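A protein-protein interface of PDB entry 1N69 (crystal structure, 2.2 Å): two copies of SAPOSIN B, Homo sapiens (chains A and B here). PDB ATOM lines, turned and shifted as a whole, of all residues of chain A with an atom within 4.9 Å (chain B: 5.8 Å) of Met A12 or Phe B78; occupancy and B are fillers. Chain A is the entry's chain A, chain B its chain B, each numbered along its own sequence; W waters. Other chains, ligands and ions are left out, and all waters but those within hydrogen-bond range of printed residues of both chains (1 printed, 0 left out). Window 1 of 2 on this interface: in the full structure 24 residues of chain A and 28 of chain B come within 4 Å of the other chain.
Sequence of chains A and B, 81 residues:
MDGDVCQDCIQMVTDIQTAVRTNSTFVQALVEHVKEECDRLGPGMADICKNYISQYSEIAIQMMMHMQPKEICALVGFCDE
The side-chain carboxylate (OD2) of Asp A15 sits close to the side-chain carboxylate (OD2) of Asp B8 (2.3 Å).
The side-chain amide nitrogen of Gln A11 lies within hydrogen-bond range of the side-chain carboxylate of Asp A15.
The side-chain sulfur (SG) of Cys B9 is disulfide-bonded to the side-chain sulfur (SG) of Cys B73 (2.0 Å).
The backbone NH (N) of Phe B78 is in hydrogen-bond range of the backbone carbonyl oxygen (O) of Cys B73.
The side-chain sulfur (SG) of Cys B6 is disulfide-bonded to the side-chain sulfur (SG) of Cys B79, at 2.0 Å.
Water W1 lies within hydrogen-bond range of the backbone carbonyl oxygen (O) of Asp B8 (2.8 Å) and the backbone carbonyl oxygen (O) of Asp A8 (2.9 Å).
Of the 11 printed residues of chain A, 7 touch a printed residue of chain B.
Hydrophobic or aromatic side chains of chain B within 4 Å of the printed part of chain A: Val B5, Met B12 and Phe B78.
Among the printed residues, no Asp or Glu carboxylate lies within 4 Å of a Lys or Arg side-chain nitrogen of the other chain.
Met A12 touches just these residues of chain B: Asp B8, Cys B9 and Phe B78.
Phe B78 touches just these residues of chain A: Met A12 (3.5 Å), Ile A16 (3.9 Å) and Leu A30 (3.8 Å).
Of the printed residues of chain B, Gln A11 touches Asp B8 (3.6 Å).
Of the printed residues of chain A, Asp B8 touches Gln A11 (3.6 Å), Met A12 (3.6 Å) and Asp A15 (2.3 Å).
Printed residues of chain B within 4 Å of Cys A9: Met B12 (3.6 Å).
Printed residues of chain A within 4 Å of Val B76: Leu A30.
Of the printed residues of chain B, Leu A30 touches Val B76 (3.1 Å), Gly B77 (3.7 Å) and Phe B78 (3.8 Å).
The nearest residue of chain B that does not touch Met A12 is Met B12 (4.1 Å).
The nearest residue of chain A that does not touch Phe B78 is Phe A26 (4.4 Å).
Asp A8 touches Met B12.
Cys A9 touches Met B12.
Gln A11 touches Asp B8 (CG to OD1, 3.6 Å).
Met A12 touches Asp B8.
Cys B9 touches Met A12.
Phe B78 touches Met A12.
Asp A15 touches Val B5 (O to CG2, 3.8 Å).
CD1 of Leu A30 touches O of Val B76, at 3.1 Å.
Leu A30 touches Gly B77.
Leu A30 touches Phe B78.
Asp A8 touches Met B12, and with the chains exchanged Met A12 touches Asp B8.
Cys A9 touches Met B12, and with the chains exchanged Met A12 touches Cys B9.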
ATOM      1  N   ASP A   8     -17.934  -7.803 -20.368  1.00  0.00           N
ATOM      2  CA  ASP A   8     -18.763  -8.958 -20.069  1.00  0.00           C
ATOM      3  C   ASP A   8     -19.438  -8.746 -18.725  1.00  0.00           C
ATOM      4  O   ASP A   8     -20.602  -9.094 -18.551  1.00  0.00           O
ATOM      5  CB  ASP A   8     -17.929 -10.256 -20.108  1.00  0.00           C
ATOM      6  CG  ASP A   8     -17.447 -10.589 -21.532  1.00  0.00           C
ATOM      7  OD1 ASP A   8     -18.118 -10.178 -22.501  1.00  0.00           O
ATOM      8  OD2 ASP A   8     -16.409 -11.257 -21.704  1.00  0.00           O
ATOM      9  N   CYS A   9     -18.737  -8.122 -17.783  1.00  0.00           N
ATOM     10  CA  CYS A   9     -19.347  -7.864 -16.480  1.00  0.00           C
ATOM     11  C   CYS A   9     -20.465  -6.819 -16.628  1.00  0.00           C
ATOM     12  O   CYS A   9     -21.566  -6.987 -16.097  1.00  0.00           O
ATOM     13  CB  CYS A   9     -18.300  -7.374 -15.470  1.00  0.00           C
ATOM     14  SG  CYS A   9     -19.073  -6.999 -13.865  1.00  0.00           S
ATOM     15  N   ILE A  10     -20.189  -5.749 -17.363  1.00  0.00           N
ATOM     16  CA  ILE A  10     -21.190  -4.706 -17.591  1.00  0.00           C
ATOM     17  C   ILE A  10     -22.446  -5.277 -18.267  1.00  0.00           C
ATOM     18  O   ILE A  10     -23.574  -4.918 -17.909  1.00  0.00           O
ATOM     19  CB  ILE A  10     -20.588  -3.562 -18.458  1.00  0.00           C
ATOM     20  CG1 ILE A  10     -19.644  -2.719 -17.592  1.00  0.00           C
ATOM     21  CG2 ILE A  10     -21.701  -2.714 -19.085  1.00  0.00           C
ATOM     22  CD1 ILE A  10     -18.794  -1.721 -18.377  1.00  0.00           C
ATOM     23  N   GLN A  11     -22.256  -6.167 -19.242  1.00  0.00           N
ATOM     24  CA  GLN A  11     -23.392  -6.775 -19.930  1.00  0.00           C
ATOM     25  C   GLN A  11     -24.216  -7.652 -18.981  1.00  0.00           C
ATOM     26  O   GLN A  11     -25.448  -7.599 -18.987  1.00  0.00           O
ATOM     27  CB  GLN A  11     -22.920  -7.614 -21.125  1.00  0.00           C
ATOM     28  CG  GLN A  11     -24.064  -8.033 -22.032  1.00  0.00           C
ATOM     29  CD  GLN A  11     -24.861  -6.834 -22.504  1.00  0.00           C
ATOM     30  OE1 GLN A  11     -24.284  -5.824 -22.915  1.00  0.00           O
ATOM     31  NE2 GLN A  11     -26.189  -6.931 -22.443  1.00  0.00           N
ATOM     32  N   MET A  12     -23.538  -8.460 -18.168  1.00  0.00           N
ATOM     33  CA  MET A  12     -24.233  -9.326 -17.225  1.00  0.00           C
ATOM     34  C   MET A  12     -25.046  -8.493 -16.224  1.00  0.00           C
ATOM     35  O   MET A  12     -26.209  -8.794 -15.953  1.00  0.00           O
ATOM     36  CB  MET A  12     -23.241 -10.221 -16.474  1.00  0.00           C
ATOM     37  CG  MET A  12     -23.926 -11.385 -15.754  1.00  0.00           C
ATOM     38  SD  MET A  12     -22.800 -12.453 -14.840  1.00  0.00           S
ATOM     39  CE  MET A  12     -23.998 -13.478 -14.042  1.00  0.00           C
ATOM     40  N   VAL A  13     -24.440  -7.441 -15.683  1.00  0.00           N
ATOM     41  CA  VAL A  13     -25.148  -6.584 -14.730  1.00  0.00           C
ATOM     42  C   VAL A  13     -26.365  -5.928 -15.391  1.00  0.00           C
ATOM     43  O   VAL A  13     -27.455  -5.891 -14.819  1.00  0.00           O
ATOM     44  CB  VAL A  13     -24.219  -5.493 -14.169  1.00  0.00           C
ATOM     45  CG1 VAL A  13     -25.028  -4.519 -13.316  1.00  0.00           C
ATOM     46  CG2 VAL A  13     -23.111  -6.138 -13.336  1.00  0.00           C
ATOM     47  N   THR A  14     -26.170  -5.429 -16.607  1.00  0.00           N
ATOM     48  CA  THR A  14     -27.238  -4.795 -17.375  1.00  0.00           C
ATOM     49  C   THR A  14     -28.414  -5.738 -17.565  1.00  0.00           C
ATOM     50  O   THR A  14     -29.570  -5.355 -17.390  1.00  0.00           O
ATOM     51  CB  THR A  14     -26.759  -4.416 -18.790  1.00  0.00           C
ATOM     52  OG1 THR A  14     -25.644  -3.527 -18.698  1.00  0.00           O
ATOM     53  CG2 THR A  14     -27.893  -3.774 -19.582  1.00  0.00           C
ATOM     54  N   ASP A  15     -28.121  -6.972 -17.956  1.00  0.00           N
ATOM     55  CA  ASP A  15     -29.181  -7.937 -18.185  1.00  0.00           C
ATOM     56  C   ASP A  15     -29.857  -8.411 -16.899  1.00  0.00           C
ATOM     57  O   ASP A  15     -31.048  -8.746 -16.906  1.00  0.00           O
ATOM     58  CB  ASP A  15     -28.648  -9.118 -18.994  1.00  0.00           C
ATOM     59  CG  ASP A  15     -28.207  -8.706 -20.388  1.00  0.00           C
ATOM     60  OD1 ASP A  15     -28.805  -7.753 -20.937  1.00  0.00           O
ATOM     61  OD2 ASP A  15     -27.274  -9.336 -20.936  1.00  0.00           O
ATOM     62  N   ILE A  16     -29.103  -8.439 -15.802  1.00  0.00           N
ATOM     63  CA  ILE A  16     -29.663  -8.834 -14.517  1.00  0.00           C
ATOM     64  C   ILE A  16     -30.621  -7.718 -14.079  1.00  0.00           C
ATOM     65  O   ILE A  16     -31.735  -7.996 -13.631  1.00  0.00           O
ATOM     66  CB  ILE A  16     -28.549  -9.056 -13.457  1.00  0.00           C
ATOM     67  CG1 ILE A  16     -27.804 -10.360 -13.770  1.00  0.00           C
ATOM     68  CG2 ILE A  16     -29.146  -9.110 -12.039  1.00  0.00           C
ATOM     69  CD1 ILE A  16     -26.619 -10.617 -12.869  1.00  0.00           C
ATOM     70  N   PHE A  26     -37.819 -13.649 -11.191  1.00  0.00           N
ATOM     71  CA  PHE A  26     -36.364 -13.755 -11.241  1.00  0.00           C
ATOM     72  C   PHE A  26     -35.614 -13.833  -9.909  1.00  0.00           C
ATOM     73  O   PHE A  26     -34.972 -14.839  -9.612  1.00  0.00           O
ATOM     74  CB  PHE A  26     -35.790 -12.600 -12.063  1.00  0.00           C
ATOM     75  CG  PHE A  26     -34.336 -12.768 -12.401  1.00  0.00           C
ATOM     76  CD1 PHE A  26     -33.927 -13.764 -13.287  1.00  0.00           C
ATOM     77  CD2 PHE A  26     -33.372 -11.940 -11.826  1.00  0.00           C
ATOM     78  CE1 PHE A  26     -32.578 -13.936 -13.598  1.00  0.00           C
ATOM     79  CE2 PHE A  26     -32.015 -12.104 -12.129  1.00  0.00           C
ATOM     80  CZ  PHE A  26     -31.618 -13.104 -13.015  1.00  0.00           C
ATOM     81  N   LEU A  30     -34.018 -17.192  -7.958  1.00  0.00           N
ATOM     82  CA  LEU A  30     -32.564 -17.240  -7.804  1.00  0.00           C
ATOM     83  C   LEU A  30     -32.135 -17.415  -6.346  1.00  0.00           C
ATOM     84  O   LEU A  30     -31.243 -18.207  -6.042  1.00  0.00           O
ATOM     85  CB  LEU A  30     -31.931 -15.968  -8.366  1.00  0.00           C
ATOM     86  CG  LEU A  30     -30.439 -15.781  -8.076  1.00  0.00           C
ATOM     87  CD1 LEU A  30     -29.642 -16.888  -8.764  1.00  0.00           C
ATOM     88  CD2 LEU A  30     -29.985 -14.410  -8.569  1.00  0.00           C
ATOM     89  N   VAL B   5     -29.076 -13.569 -19.423  1.00  0.00           N
ATOM     90  CA  VAL B   5     -28.320 -13.758 -18.182  1.00  0.00           C
ATOM     91  C   VAL B   5     -27.498 -15.051 -18.116  1.00  0.00           C
ATOM     92  O   VAL B   5     -26.345 -15.030 -17.678  1.00  0.00           O
ATOM     93  CB  VAL B   5     -29.253 -13.695 -16.945  1.00  0.00           C
ATOM     94  CG1 VAL B   5     -28.502 -14.151 -15.687  1.00  0.00           C
ATOM     95  CG2 VAL B   5     -29.755 -12.277 -16.765  1.00  0.00           C
ATOM     96  N   CYS B   6     -28.075 -16.170 -18.540  1.00  0.00           N
ATOM     97  CA  CYS B   6     -27.337 -17.428 -18.507  1.00  0.00           C
ATOM     98  C   CYS B   6     -26.098 -17.371 -19.410  1.00  0.00           C
ATOM     99  O   CYS B   6     -25.007 -17.760 -18.993  1.00  0.00           O
ATOM    100  CB  CYS B   6     -28.249 -18.600 -18.905  1.00  0.00           C
ATOM    101  SG  CYS B   6     -27.349 -20.152 -19.225  1.00  0.00           S
ATOM    102  N   GLN B   7     -26.259 -16.888 -20.644  1.00  0.00           N
ATOM    103  CA  GLN B   7     -25.120 -16.774 -21.549  1.00  0.00           C
ATOM    104  C   GLN B   7     -24.128 -15.753 -20.993  1.00  0.00           C
ATOM    105  O   GLN B   7     -22.912 -15.970 -21.061  1.00  0.00           O
ATOM    106  CB  GLN B   7     -25.582 -16.379 -22.966  1.00  0.00           C
ATOM    107  CG  GLN B   7     -26.240 -17.530 -23.738  1.00  0.00           C
ATOM    108  CD  GLN B   7     -25.307 -18.737 -23.888  1.00  0.00           C
ATOM    109  OE1 GLN B   7     -24.101 -18.578 -24.076  1.00  0.00           O
ATOM    110  NE2 GLN B   7     -25.864 -19.941 -23.804  1.00  0.00           N
ATOM    111  N   ASP B   8     -24.630 -14.650 -20.427  1.00  0.00           N
ATOM    112  CA  ASP B   8     -23.730 -13.647 -19.834  1.00  0.00           C
ATOM    113  C   ASP B   8     -22.892 -14.315 -18.743  1.00  0.00           C
ATOM    114  O   ASP B   8     -21.681 -14.093 -18.640  1.00  0.00           O
ATOM    115  CB  ASP B   8     -24.492 -12.489 -19.169  1.00  0.00           C
ATOM    116  CG  ASP B   8     -25.245 -11.612 -20.156  1.00  0.00           C
ATOM    117  OD1 ASP B   8     -24.780 -11.454 -21.314  1.00  0.00           O
ATOM    118  OD2 ASP B   8     -26.295 -11.050 -19.747  1.00  0.00           O
ATOM    119  N   CYS B   9     -23.540 -15.123 -17.906  1.00  0.00           N
ATOM    120  CA  CYS B   9     -22.811 -15.789 -16.838  1.00  0.00           C
ATOM    121  C   CYS B   9     -21.748 -16.748 -17.383  1.00  0.00           C
ATOM    122  O   CYS B   9     -20.614 -16.783 -16.902  1.00  0.00           O
ATOM    123  CB  CYS B   9     -23.779 -16.536 -15.909  1.00  0.00           C
ATOM    124  SG  CYS B   9     -22.936 -17.338 -14.497  1.00  0.00           S
ATOM    125  N   MET B  12     -18.876 -14.681 -18.751  1.00  0.00           N
ATOM    126  CA  MET B  12     -18.220 -14.037 -17.621  1.00  0.00           C
ATOM    127  C   MET B  12     -17.332 -15.007 -16.865  1.00  0.00           C
ATOM    128  O   MET B  12     -16.171 -14.701 -16.575  1.00  0.00           O
ATOM    129  CB  MET B  12     -19.280 -13.467 -16.677  1.00  0.00           C
ATOM    130  CG  MET B  12     -18.778 -13.021 -15.329  1.00  0.00           C
ATOM    131  SD  MET B  12     -18.797 -11.234 -15.236  1.00  0.00           S
ATOM    132  CE  MET B  12     -17.355 -10.979 -16.186  1.00  0.00           C
ATOM    133  N   CYS B  73     -22.361 -21.687 -13.355  1.00  0.00           N
ATOM    134  CA  CYS B  73     -23.541 -20.847 -13.514  1.00  0.00           C
ATOM    135  C   CYS B  73     -24.841 -21.572 -13.155  1.00  0.00           C
ATOM    136  O   CYS B  73     -25.810 -20.940 -12.753  1.00  0.00           O
ATOM    137  CB  CYS B  73     -23.600 -20.291 -14.942  1.00  0.00           C
ATOM    138  SG  CYS B  73     -22.256 -19.103 -15.277  1.00  0.00           S
ATOM    139  N   ALA B  74     -24.854 -22.893 -13.306  1.00  0.00           N
ATOM    140  CA  ALA B  74     -26.025 -23.701 -12.959  1.00  0.00           C
ATOM    141  C   ALA B  74     -26.097 -23.743 -11.439  1.00  0.00           C
ATOM    142  O   ALA B  74     -27.159 -23.585 -10.847  1.00  0.00           O
ATOM    143  CB  ALA B  74     -25.883 -25.128 -13.522  1.00  0.00           C
ATOM    144  N   VAL B  76     -24.937 -21.567  -9.175  1.00  0.00           N
ATOM    145  CA  VAL B  76     -25.353 -20.273  -8.634  1.00  0.00           C
ATOM    146  C   VAL B  76     -26.758 -19.826  -9.037  1.00  0.00           C
ATOM    147  O   VAL B  76     -27.292 -18.864  -8.479  1.00  0.00           O
ATOM    148  CB  VAL B  76     -24.337 -19.169  -9.020  1.00  0.00           C
ATOM    149  CG1 VAL B  76     -24.654 -17.874  -8.286  1.00  0.00           C
ATOM    150  CG2 VAL B  76     -22.928 -19.630  -8.682  1.00  0.00           C
ATOM    151  N   GLY B  77     -27.356 -20.497 -10.015  1.00  0.00           N
ATOM    152  CA  GLY B  77     -28.711 -20.147 -10.404  1.00  0.00           C
ATOM    153  C   GLY B  77     -28.949 -19.254 -11.609  1.00  0.00           C
ATOM    154  O   GLY B  77     -30.090 -18.866 -11.854  1.00  0.00           O
ATOM    155  N   PHE B  78     -27.907 -18.912 -12.359  1.00  0.00           N
ATOM    156  CA  PHE B  78     -28.089 -18.062 -13.538  1.00  0.00           C
ATOM    157  C   PHE B  78     -28.427 -18.859 -14.797  1.00  0.00           C
ATOM    158  O   PHE B  78     -28.902 -18.303 -15.783  1.00  0.00           O
ATOM    159  CB  PHE B  78     -26.841 -17.203 -13.767  1.00  0.00           C
ATOM    160  CG  PHE B  78     -26.687 -16.092 -12.764  1.00  0.00           C
ATOM    161  CD1 PHE B  78     -25.517 -15.959 -12.024  1.00  0.00           C
ATOM    162  CD2 PHE B  78     -27.740 -15.204 -12.527  1.00  0.00           C
ATOM    163  CE1 PHE B  78     -25.396 -14.955 -11.051  1.00  0.00           C
ATOM    164  CE2 PHE B  78     -27.632 -14.200 -11.562  1.00  0.00           C
ATOM    165  CZ  PHE B  78     -26.459 -14.076 -10.820  1.00  0.00           C
ATOM    166  N   CYS B  79     -28.176 -20.164 -14.764  1.00  0.00           N
ATOM    167  CA  CYS B  79     -28.485 -21.026 -15.897  1.00  0.00           C
ATOM    168  C   CYS B  79     -29.394 -22.161 -15.466  1.00  0.00           C
ATOM    169  O   CYS B  79     -29.334 -22.604 -14.323  1.00  0.00           O
ATOM    170  CB  CYS B  79     -27.216 -21.618 -16.513  1.00  0.00           C
ATOM    171  SG  CYS B  79     -26.232 -20.481 -17.539  1.00  0.00           S
ATOM    172  N   ASP B  80     -30.216 -22.618 -16.410  1.00  0.00           N
ATOM    173  CA  ASP B  80     -31.197 -23.694 -16.247  1.00  0.00           C
ATOM    174  C   ASP B  80     -32.583 -23.119 -16.002  1.00  0.00           C
ATOM    175  O   ASP B  80     -33.456 -23.349 -16.862  1.00  0.00           O
ATOM    176  CB  ASP B  80     -30.831 -24.643 -15.103  1.00  0.00           C
ATOM    177  CG  ASP B  80     -29.716 -25.597 -15.469  1.00  0.00           C
ATOM    178  OD1 ASP B  80     -29.505 -26.565 -14.710  1.00  0.00           O
ATOM    179  OD2 ASP B  80     -29.052 -25.381 -16.508  1.00  0.00           O
HETATM  180  O   HOH W   1     -21.291 -11.601 -19.792  1.00  0.00           O
